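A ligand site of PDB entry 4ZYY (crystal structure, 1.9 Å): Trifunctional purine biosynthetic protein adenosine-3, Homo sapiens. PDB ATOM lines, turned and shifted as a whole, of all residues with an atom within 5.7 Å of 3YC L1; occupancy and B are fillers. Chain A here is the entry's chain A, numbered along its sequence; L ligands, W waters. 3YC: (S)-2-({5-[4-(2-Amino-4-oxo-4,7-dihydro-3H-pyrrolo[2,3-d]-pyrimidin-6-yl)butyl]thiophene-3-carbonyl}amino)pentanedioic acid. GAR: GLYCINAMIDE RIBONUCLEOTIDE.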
ATOM      1  N   ASN A  37      -4.787  14.144  12.407  1.00  0.00           N
ATOM      2  CA  ASN A  37      -3.760  14.351  13.426  1.00  0.00           C
ATOM      3  C   ASN A  37      -2.886  15.540  13.069  1.00  0.00           C
ATOM      4  O   ASN A  37      -1.978  15.896  13.818  1.00  0.00           O
ATOM      5  CB  ASN A  37      -2.897  13.094  13.607  1.00  0.00           C
ATOM      6  CG  ASN A  37      -2.046  12.790  12.394  1.00  0.00           C
ATOM      7  OD1 ASN A  37      -2.554  12.604  11.286  1.00  0.00           O
ATOM      8  ND2 ASN A  37      -0.734  12.739  12.594  1.00  0.00           N
ATOM      9  N   LYS A  38      -3.159  16.146  11.916  1.00  0.00           N
ATOM     10  CA  LYS A  38      -2.356  17.260  11.421  1.00  0.00           C
ATOM     11  C   LYS A  38      -3.226  18.416  10.946  1.00  0.00           C
ATOM     12  O   LYS A  38      -4.227  18.218  10.266  1.00  0.00           O
ATOM     13  CB  LYS A  38      -1.424  16.786  10.296  1.00  0.00           C
ATOM     14  CG  LYS A  38      -0.340  15.828  10.772  1.00  0.00           C
ATOM     15  CD  LYS A  38       0.589  15.400   9.645  1.00  0.00           C
ATOM     16  CE  LYS A  38       1.650  14.415  10.162  1.00  0.00           C
ATOM     17  NZ  LYS A  38       2.549  15.005  11.203  1.00  0.00           N
ATOM     18  N   HIS A  59      -1.286  14.858  17.635  1.00  0.00           N
ATOM     19  CA  HIS A  59      -0.536  13.864  18.408  1.00  0.00           C
ATOM     20  C   HIS A  59       0.662  14.477  19.125  1.00  0.00           C
ATOM     21  O   HIS A  59       1.186  13.880  20.073  1.00  0.00           O
ATOM     22  CB  HIS A  59      -0.080  12.713  17.500  1.00  0.00           C
ATOM     23  CG  HIS A  59       0.941  13.110  16.471  1.00  0.00           C
ATOM     24  ND1 HIS A  59       0.594  13.557  15.220  1.00  0.00           N
ATOM     25  CD2 HIS A  59       2.298  13.128  16.515  1.00  0.00           C
ATOM     26  CE1 HIS A  59       1.695  13.830  14.528  1.00  0.00           C
ATOM     27  NE2 HIS A  59       2.737  13.571  15.294  1.00  0.00           N
ATOM     28  N   LYS A  60       1.081  15.655  18.676  1.00  0.00           N
ATOM     29  CA  LYS A  60       2.226  16.360  19.273  1.00  0.00           C
ATOM     30  C   LYS A  60       1.938  16.903  20.672  1.00  0.00           C
ATOM     31  O   LYS A  60       2.837  17.393  21.347  1.00  0.00           O
ATOM     32  CB  LYS A  60       2.660  17.515  18.369  1.00  0.00           C
ATOM     33  CG  LYS A  60       3.224  17.093  17.035  1.00  0.00           C
ATOM     34  CD  LYS A  60       4.385  16.133  17.192  1.00  0.00           C
ATOM     35  CE  LYS A  60       5.332  16.226  16.010  1.00  0.00           C
ATOM     36  NZ  LYS A  60       5.519  14.901  15.348  1.00  0.00           N
ATOM     37  N   ARG A  65       1.179   7.438  23.035  1.00  0.00           N
ATOM     38  CA  ARG A  65       0.274   6.918  22.031  1.00  0.00           C
ATOM     39  C   ARG A  65      -1.123   6.628  22.620  1.00  0.00           C
ATOM     40  O   ARG A  65      -2.145   6.906  21.988  1.00  0.00           O
ATOM     41  CB  ARG A  65       0.866   5.652  21.410  1.00  0.00           C
ATOM     42  CG  ARG A  65       0.305   5.291  20.052  1.00  0.00           C
ATOM     43  CD  ARG A  65       1.098   4.165  19.399  1.00  0.00           C
ATOM     44  NE  ARG A  65       2.500   4.497  19.147  1.00  0.00           N
ATOM     45  CZ  ARG A  65       2.963   5.104  18.057  1.00  0.00           C
ATOM     46  NH1 ARG A  65       2.135   5.468  17.081  1.00  0.00           N
ATOM     47  NH2 ARG A  65       4.256   5.359  17.936  1.00  0.00           N
ATOM     48  N   LEU A  86      -9.182   4.388   8.160  1.00  0.00           N
ATOM     49  CA  LEU A  86      -7.898   5.095   8.146  1.00  0.00           C
ATOM     50  C   LEU A  86      -7.572   5.383   6.684  1.00  0.00           C
ATOM     51  O   LEU A  86      -7.317   4.465   5.914  1.00  0.00           O
ATOM     52  CB  LEU A  86      -6.795   4.264   8.811  1.00  0.00           C
ATOM     53  CG  LEU A  86      -7.114   3.728  10.214  1.00  0.00           C
ATOM     54  CD1 LEU A  86      -5.873   3.092  10.845  1.00  0.00           C
ATOM     55  CD2 LEU A  86      -7.657   4.824  11.122  1.00  0.00           C
ATOM     56  N   PHE A  89      -4.109   8.091   7.009  1.00  0.00           N
ATOM     57  CA  PHE A  89      -3.743   8.353   8.406  1.00  0.00           C
ATOM     58  C   PHE A  89      -2.448   7.618   8.714  1.00  0.00           C
ATOM     59  O   PHE A  89      -2.370   6.400   8.568  1.00  0.00           O
ATOM     60  CB  PHE A  89      -4.872   7.894   9.332  1.00  0.00           C
ATOM     61  CG  PHE A  89      -4.639   8.192  10.787  1.00  0.00           C
ATOM     62  CD1 PHE A  89      -4.817   9.469  11.290  1.00  0.00           C
ATOM     63  CD2 PHE A  89      -4.300   7.164  11.661  1.00  0.00           C
ATOM     64  CE1 PHE A  89      -4.643   9.736  12.644  1.00  0.00           C
ATOM     65  CE2 PHE A  89      -4.127   7.419  13.020  1.00  0.00           C
ATOM     66  CZ  PHE A  89      -4.291   8.705  13.514  1.00  0.00           C
ATOM     67  N   MET A  90      -1.414   8.350   9.146  1.00  0.00           N
ATOM     68  CA  MET A  90      -0.079   7.749   9.209  1.00  0.00           C
ATOM     69  C   MET A  90       0.452   7.464  10.610  1.00  0.00           C
ATOM     70  O   MET A  90       1.669   7.363  10.801  1.00  0.00           O
ATOM     71  CB  MET A  90       0.925   8.648   8.467  1.00  0.00           C
ATOM     72  CG  MET A  90       0.669   8.821   6.970  1.00  0.00           C
ATOM     73  SD  MET A  90       0.491   7.272   6.029  1.00  0.00           S
ATOM     74  CE  MET A  90       2.127   6.562   6.247  1.00  0.00           C
ATOM     75  N   ARG A  91      -0.436   7.304  11.593  1.00  0.00           N
ATOM     76  CA  ARG A  91       0.004   6.934  12.937  1.00  0.00           C
ATOM     77  C   ARG A  91      -0.259   5.468  13.229  1.00  0.00           C
ATOM     78  O   ARG A  91      -1.300   4.923  12.842  1.00  0.00           O
ATOM     79  CB  ARG A  91      -0.709   7.784  14.012  1.00  0.00           C
ATOM     80  CG  ARG A  91      -0.679   9.269  13.772  1.00  0.00           C
ATOM     81  CD  ARG A  91       0.702   9.809  13.976  1.00  0.00           C
ATOM     82  NE  ARG A  91       1.203   9.465  15.295  1.00  0.00           N
ATOM     83  CZ  ARG A  91       2.425   9.771  15.715  1.00  0.00           C
ATOM     84  NH1 ARG A  91       3.263  10.430  14.921  1.00  0.00           N
ATOM     85  NH2 ARG A  91       2.814   9.421  16.938  1.00  0.00           N
ATOM     86  N   ILE A  92       0.671   4.824  13.932  1.00  0.00           N
ATOM     87  CA  ILE A  92       0.428   3.504  14.498  1.00  0.00           C
ATOM     88  C   ILE A  92      -0.476   3.618  15.718  1.00  0.00           C
ATOM     89  O   ILE A  92      -0.233   4.433  16.598  1.00  0.00           O
ATOM     90  CB  ILE A  92       1.750   2.824  14.879  1.00  0.00           C
ATOM     91  CG1 ILE A  92       2.572   2.559  13.620  1.00  0.00           C
ATOM     92  CG2 ILE A  92       1.494   1.539  15.645  1.00  0.00           C
ATOM     93  CD1 ILE A  92       3.910   1.946  13.903  1.00  0.00           C
ATOM     94  N   LEU A  93      -1.528   2.801  15.779  1.00  0.00           N
ATOM     95  CA  LEU A  93      -2.488   2.863  16.882  1.00  0.00           C
ATOM     96  C   LEU A  93      -2.153   1.866  17.987  1.00  0.00           C
ATOM     97  O   LEU A  93      -1.661   0.766  17.721  1.00  0.00           O
ATOM     98  CB  LEU A  93      -3.897   2.599  16.359  1.00  0.00           C
ATOM     99  CG  LEU A  93      -4.366   3.619  15.317  1.00  0.00           C
ATOM    100  CD1 LEU A  93      -5.535   3.044  14.516  1.00  0.00           C
ATOM    101  CD2 LEU A  93      -4.776   4.898  16.024  1.00  0.00           C
ATOM    102  N   SER A  94      -2.442   2.259  19.220  1.00  0.00           N
ATOM    103  CA  SER A  94      -2.146   1.418  20.371  1.00  0.00           C
ATOM    104  C   SER A  94      -2.982   0.155  20.405  1.00  0.00           C
ATOM    105  O   SER A  94      -4.091   0.120  19.879  1.00  0.00           O
ATOM    106  CB  SER A  94      -2.365   2.203  21.672  1.00  0.00           C
ATOM    107  OG  SER A  94      -3.759   2.386  21.886  1.00  0.00           O
ATOM    108  N   VAL A  98      -6.933  -0.513  19.234  1.00  0.00           N
ATOM    109  CA  VAL A  98      -7.130  -1.485  18.168  1.00  0.00           C
ATOM    110  C   VAL A  98      -8.065  -2.615  18.613  1.00  0.00           C
ATOM    111  O   VAL A  98      -8.946  -3.037  17.863  1.00  0.00           O
ATOM    112  CB  VAL A  98      -5.782  -2.079  17.698  1.00  0.00           C
ATOM    113  CG1 VAL A  98      -5.994  -3.289  16.820  1.00  0.00           C
ATOM    114  CG2 VAL A  98      -4.955  -1.018  16.982  1.00  0.00           C
ATOM    115  N   ASN A 107      -8.228  -0.084   6.997  1.00  0.00           N
ATOM    116  CA  ASN A 107      -7.085   0.703   6.550  1.00  0.00           C
ATOM    117  C   ASN A 107      -6.822   0.450   5.077  1.00  0.00           C
ATOM    118  O   ASN A 107      -7.021  -0.675   4.611  1.00  0.00           O
ATOM    119  CB  ASN A 107      -5.833   0.380   7.370  1.00  0.00           C
ATOM    120  CG  ASN A 107      -4.621   1.175   6.913  1.00  0.00           C
ATOM    121  OD1 ASN A 107      -4.647   2.409   6.929  1.00  0.00           O
ATOM    122  ND2 ASN A 107      -3.550   0.479   6.520  1.00  0.00           N
ATOM    123  N   GLY A 118       4.508  -1.256   5.806  1.00  0.00           N
ATOM    124  CA  GLY A 118       5.198  -0.075   6.299  1.00  0.00           C
ATOM    125  C   GLY A 118       4.799   1.207   5.596  1.00  0.00           C
ATOM    126  O   GLY A 118       3.836   1.243   4.823  1.00  0.00           O
ATOM    127  N   SER A 119       5.544   2.270   5.852  1.00  0.00           N
ATOM    128  CA  SER A 119       5.094   3.606   5.473  1.00  0.00           C
ATOM    129  C   SER A 119       5.600   4.061   4.117  1.00  0.00           C
ATOM    130  O   SER A 119       5.201   5.128   3.644  1.00  0.00           O
ATOM    131  CB  SER A 119       5.527   4.610   6.538  1.00  0.00           C
ATOM    132  OG  SER A 119       6.932   4.636   6.581  1.00  0.00           O
ATOM    133  N   HIS A 138      -7.726  -3.608   4.544  1.00  0.00           N
ATOM    134  CA  HIS A 138      -7.717  -4.676   5.532  1.00  0.00           C
ATOM    135  C   HIS A 138      -8.289  -4.200   6.862  1.00  0.00           C
ATOM    136  O   HIS A 138      -8.247  -3.017   7.162  1.00  0.00           O
ATOM    137  CB  HIS A 138      -6.287  -5.199   5.733  1.00  0.00           C
ATOM    138  CG  HIS A 138      -5.339  -4.160   6.261  1.00  0.00           C
ATOM    139  ND1 HIS A 138      -5.062  -4.029   7.603  1.00  0.00           N
ATOM    140  CD2 HIS A 138      -4.622  -3.203   5.628  1.00  0.00           C
ATOM    141  CE1 HIS A 138      -4.206  -3.029   7.785  1.00  0.00           C
ATOM    142  NE2 HIS A 138      -3.920  -2.517   6.599  1.00  0.00           N
ATOM    143  N   PHE A 139      -8.796  -5.134   7.658  1.00  0.00           N
ATOM    144  CA  PHE A 139      -9.105  -4.807   9.046  1.00  0.00           C
ATOM    145  C   PHE A 139      -7.814  -4.501   9.801  1.00  0.00           C
ATOM    146  O   PHE A 139      -6.785  -5.134   9.566  1.00  0.00           O
ATOM    147  CB  PHE A 139      -9.835  -5.948   9.734  1.00  0.00           C
ATOM    148  CG  PHE A 139     -11.276  -6.060   9.347  1.00  0.00           C
ATOM    149  CD1 PHE A 139     -12.178  -5.086   9.769  1.00  0.00           C
ATOM    150  CD2 PHE A 139     -11.718  -7.093   8.571  1.00  0.00           C
ATOM    151  CE1 PHE A 139     -13.514  -5.176   9.442  1.00  0.00           C
ATOM    152  CE2 PHE A 139     -13.071  -7.206   8.236  1.00  0.00           C
ATOM    153  CZ  PHE A 139     -13.964  -6.238   8.667  1.00  0.00           C
ATOM    154  N   VAL A 140      -7.876  -3.525  10.695  1.00  0.00           N
ATOM    155  CA  VAL A 140      -6.703  -3.152  11.457  1.00  0.00           C
ATOM    156  C   VAL A 140      -6.524  -4.053  12.680  1.00  0.00           C
ATOM    157  O   VAL A 140      -7.416  -4.150  13.530  1.00  0.00           O
ATOM    158  CB  VAL A 140      -6.779  -1.682  11.908  1.00  0.00           C
ATOM    159  CG1 VAL A 140      -5.632  -1.353  12.857  1.00  0.00           C
ATOM    160  CG2 VAL A 140      -6.753  -0.766  10.704  1.00  0.00           C
ATOM    161  N   ALA A 141      -5.375  -4.728  12.737  1.00  0.00           N
ATOM    162  CA  ALA A 141      -5.002  -5.531  13.899  1.00  0.00           C
ATOM    163  C   ALA A 141      -3.825  -4.837  14.576  1.00  0.00           C
ATOM    164  O   ALA A 141      -3.288  -3.873  14.043  1.00  0.00           O
ATOM    165  CB  ALA A 141      -4.653  -6.944  13.468  1.00  0.00           C
ATOM    166  N   GLU A 142      -3.406  -5.313  15.747  1.00  0.00           N
ATOM    167  CA  GLU A 142      -2.343  -4.597  16.456  1.00  0.00           C
ATOM    168  C   GLU A 142      -1.056  -4.614  15.652  1.00  0.00           C
ATOM    169  O   GLU A 142      -0.378  -3.599  15.531  1.00  0.00           O
ATOM    170  CB  GLU A 142      -2.088  -5.180  17.850  1.00  0.00           C
ATOM    171  CG  GLU A 142      -0.971  -4.441  18.562  1.00  0.00           C
ATOM    172  CD  GLU A 142      -0.868  -4.749  20.046  1.00  0.00           C
ATOM    173  OE1 GLU A 142      -1.462  -5.754  20.493  1.00  0.00           O
ATOM    174  OE2 GLU A 142      -0.188  -3.982  20.749  1.00  0.00           O
ATOM    175  N   ASP A 143      -0.735  -5.777  15.083  1.00  0.00           N
ATOM    176  CA  ASP A 143       0.418  -5.883  14.195  1.00  0.00           C
ATOM    177  C   ASP A 143       0.169  -5.101  12.916  1.00  0.00           C
ATOM    178  O   ASP A 143      -0.803  -5.354  12.208  1.00  0.00           O
ATOM    179  CB  ASP A 143       0.705  -7.356  13.880  1.00  0.00           C
ATOM    180  CG  ASP A 143       2.041  -7.548  13.214  1.00  0.00           C
ATOM    181  OD1 ASP A 143       2.906  -6.664  13.362  1.00  0.00           O
ATOM    182  OD2 ASP A 143       2.224  -8.603  12.556  1.00  0.00           O
ATOM    183  N   VAL A 144       1.045  -4.134  12.620  1.00  0.00           N
ATOM    184  CA  VAL A 144       0.818  -3.223  11.518  1.00  0.00           C
ATOM    185  C   VAL A 144       0.767  -3.923  10.150  1.00  0.00           C
ATOM    186  O   VAL A 144       1.648  -4.715   9.826  1.00  0.00           O
ATOM    187  CB  VAL A 144       1.880  -2.111  11.503  1.00  0.00           C
ATOM    188  CG1 VAL A 144       1.714  -1.212  10.298  1.00  0.00           C
ATOM    189  CG2 VAL A 144       1.789  -1.304  12.774  1.00  0.00           C
ATOM    190  N   ASP A 145      -0.279  -3.619   9.381  1.00  0.00           N
ATOM    191  CA  ASP A 145      -0.482  -4.155   8.037  1.00  0.00           C
ATOM    192  C   ASP A 145      -0.595  -5.681   8.008  1.00  0.00           C
ATOM    193  O   ASP A 145      -0.302  -6.312   6.990  1.00  0.00           O
ATOM    194  CB  ASP A 145       0.637  -3.691   7.080  1.00  0.00           C
ATOM    195  CG  ASP A 145       0.676  -2.174   6.905  1.00  0.00           C
ATOM    196  OD1 ASP A 145      -0.361  -1.511   7.134  1.00  0.00           O
ATOM    197  OD2 ASP A 145       1.741  -1.648   6.545  1.00  0.00           O
ATOM    198  N   ALA A 146      -1.039  -6.274   9.120  1.00  0.00           N
ATOM    199  CA  ALA A 146      -1.147  -7.733   9.204  1.00  0.00           C
ATOM    200  C   ALA A 146      -2.595  -8.203   9.418  1.00  0.00           C
ATOM    201  O   ALA A 146      -2.854  -9.406   9.427  1.00  0.00           O
ATOM    202  CB  ALA A 146      -0.257  -8.265  10.322  1.00  0.00           C
ATOM    203  N   GLY A 147      -3.518  -7.267   9.587  1.00  0.00           N
ATOM    204  CA  GLY A 147      -4.913  -7.620   9.807  1.00  0.00           C
ATOM    205  C   GLY A 147      -5.585  -8.261   8.592  1.00  0.00           C
ATOM    206  O   GLY A 147      -5.020  -8.303   7.498  1.00  0.00           O
HETATM  207  N1  3YC L   1      -1.890   0.663  13.640  1.00  0.00           N
HETATM  208  C2  3YC L   1      -1.910  -0.634  13.929  1.00  0.00           C
HETATM  209  N3  3YC L   1      -2.103  -1.540  12.954  1.00  0.00           N
HETATM  210  C4  3YC L   1      -2.272  -1.182  11.665  1.00  0.00           C
HETATM  211  N5  3YC L   1      -2.066   2.316  11.871  1.00  0.00           N
HETATM  212  C6  3YC L   1      -2.260   2.263  10.546  1.00  0.00           C
HETATM  213  C7  3YC L   1      -2.389   0.936  10.161  1.00  0.00           C
HETATM  214  C8  3YC L   1      -2.252   0.173  11.347  1.00  0.00           C
HETATM  215  C9  3YC L   1      -2.051   1.087  12.384  1.00  0.00           C
HETATM  216  O10 3YC L   1      -2.427  -2.047  10.809  1.00  0.00           O
HETATM  217  N11 3YC L   1      -1.733  -1.067  15.284  1.00  0.00           N
HETATM  218  C12 3YC L   1       2.923   4.440   9.896  1.00  0.00           C
HETATM  219  C13 3YC L   1       4.150   4.055  10.496  1.00  0.00           C
HETATM  220  C14 3YC L   1       4.618   2.829  10.156  1.00  0.00           C
HETATM  221  S15 3YC L   1       3.473   2.186   9.059  1.00  0.00           S
HETATM  222  C16 3YC L   1       2.409   3.512   9.047  1.00  0.00           C
HETATM  223  C17 3YC L   1       4.816   4.918  11.436  1.00  0.00           C
HETATM  224  O18 3YC L   1       5.944   4.638  11.816  1.00  0.00           O
HETATM  225  N19 3YC L   1       4.130   6.081  11.916  1.00  0.00           N
HETATM  226  C20 3YC L   1       4.670   6.945  12.808  1.00  0.00           C
HETATM  227  C21 3YC L   1       4.193   8.256  12.530  1.00  0.00           C
HETATM  228  C22 3YC L   1       5.143   8.982  11.641  1.00  0.00           C
HETATM  229  C23 3YC L   1       4.416  10.116  10.995  1.00  0.00           C
HETATM  230  O24 3YC L   1       3.799  10.964  11.697  1.00  0.00           O
HETATM  231  O25 3YC L   1       4.418  10.228   9.735  1.00  0.00           O
HETATM  232  C26 3YC L   1       4.266   6.612  14.125  1.00  0.00           C
HETATM  233  O27 3YC L   1       5.119   6.644  15.062  1.00  0.00           O
HETATM  234  O28 3YC L   1       3.081   6.290  14.391  1.00  0.00           O
HETATM  235  C29 3YC L   1      -2.334   3.448   9.651  1.00  0.00           C
HETATM  236  C30 3YC L   1      -1.241   3.346   8.652  1.00  0.00           C
HETATM  237  C31 3YC L   1       0.044   3.703   9.302  1.00  0.00           C
HETATM  238  C32 3YC L   1       1.138   3.647   8.287  1.00  0.00           C
HETATM  239  C1  GAR L   2      -2.630   6.614   0.032  1.00  0.00           C
HETATM  240  O6  GAR L   2      -1.902   6.150  -1.109  1.00  0.00           O
HETATM  241  C2  GAR L   2      -2.604   5.522   1.066  1.00  0.00           C
HETATM  242  O8  GAR L   2      -2.646   4.221   0.509  1.00  0.00           O
HETATM  243  C3  GAR L   2      -1.261   5.751   1.744  1.00  0.00           C
HETATM  244  O4  GAR L   2      -1.165   7.172   1.815  1.00  0.00           O
HETATM  245  C5  GAR L   2      -1.862   7.745   0.701  1.00  0.00           C
HETATM  246  C10 GAR L   2      -2.815   8.820   1.203  1.00  0.00           C
HETATM  247  O12 GAR L   2      -3.410   9.543   0.120  1.00  0.00           O
HETATM  248  N19 GAR L   2      -1.248   5.139   3.048  1.00  0.00           N
HETATM  249  C21 GAR L   2      -0.195   4.468   3.500  1.00  0.00           C
HETATM  250  O22 GAR L   2       0.885   4.423   2.910  1.00  0.00           O
HETATM  251  C23 GAR L   2      -0.434   3.778   4.816  1.00  0.00           C
HETATM  252  N24 GAR L   2       0.640   2.866   5.155  1.00  0.00           N
HETATM  253  P15 GAR L   2      -4.713  10.464   0.348  1.00  0.00           P
HETATM  254  O16 GAR L   2      -5.767   9.456   0.702  1.00  0.00           O
HETATM  255  O17 GAR L   2      -4.860  11.191  -0.970  1.00  0.00           O
HETATM  256  O18 GAR L   2      -4.383  11.395   1.516  1.00  0.00           O
HETATM  257  O   HOH W   1       1.212  11.348  10.671  1.00  0.00           O
HETATM  258  O   HOH W   2      -3.076  -4.710  10.901  1.00  0.00           O
HETATM  259  O   HOH W   3       1.981  11.965   8.093  1.00  0.00           O
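Residues that only touch 3YC L1: Phe 89 (3.1 Å), Val 144 (3.5 Å), Val 140 (3.5 Å), Val 98 (3.6 Å), His 138 (3.6 Å), Leu 86 (3.7 Å), Asn 107 (3.7 Å), Ser 119 (3.8 Å), Gly 118 (3.8 Å) and Asp 143 (3.9 Å). Hydrophobic or aromatic side chains within 4 Å of 3YC L1: Leu 86, Met 90, Ile 92, Leu 93, Val 98, His 138, Val 140 and Val 144. Along chain A the residues within 4 Å of 3YC L1 span positions 65 to 145. The nearest printed residue that does not touch 3YC L1 is Lys 38 (4.3 Å).
The backbone carbonyl oxygen (O) of Arg 91 lies within hydrogen-bond range of a nitrogen (N5) of 3YC L1, at 2.9 Å. N of Leu 93 sits at hydrogen-bond distance from N1 of 3YC L1. NH1 of Arg 65 is in salt-bridge range of O28 of 3YC L1, 3.0 Å away. The backbone carbonyl oxygen (O) of Met 90 lies within hydrogen-bond range of a nitrogen (N19) of 3YC L1. The backbone carbonyl oxygen of Ala 141 sits at hydrogen-bond distance from a nitrogen (N3) of 3YC L1 (2.8 Å). O of Leu 93 is in hydrogen-bond range of N11 of 3YC L1. The backbone NH of Ile 92 is in hydrogen-bond range of an oxygen (O28) of 3YC L1. O24 of 3YC L1 lies within salt-bridge range of NH1 of Arg 91 (3.3 Å). The backbone NH (N) of Asp 145 lies within hydrogen-bond range of an oxygen (O10) of 3YC L1. N11 of 3YC L1 is in hydrogen-bond range of O of Glu 142 (2.9 Å).
OD2 of Asp 145 lies within hydrogen-bond range of N of Gly 118, at 2.9 Å. The guanidinium group (NH1) of Arg 65 sits at hydrogen-bond distance from the backbone carbonyl oxygen (O) of Ile 92 (2.6 Å). The backbone NH (N) of Asn 107 sits at hydrogen-bond distance from the backbone carbonyl oxygen (O) of His 138, at 2.9 Å. NE2 of His 59 sits at hydrogen-bond distance from NH1 of Arg 91, at 3.2 Å.
Water W1 lies within hydrogen-bond range of an oxygen (O24) of 3YC L1 and the side-chain amide nitrogen of Asn 37.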
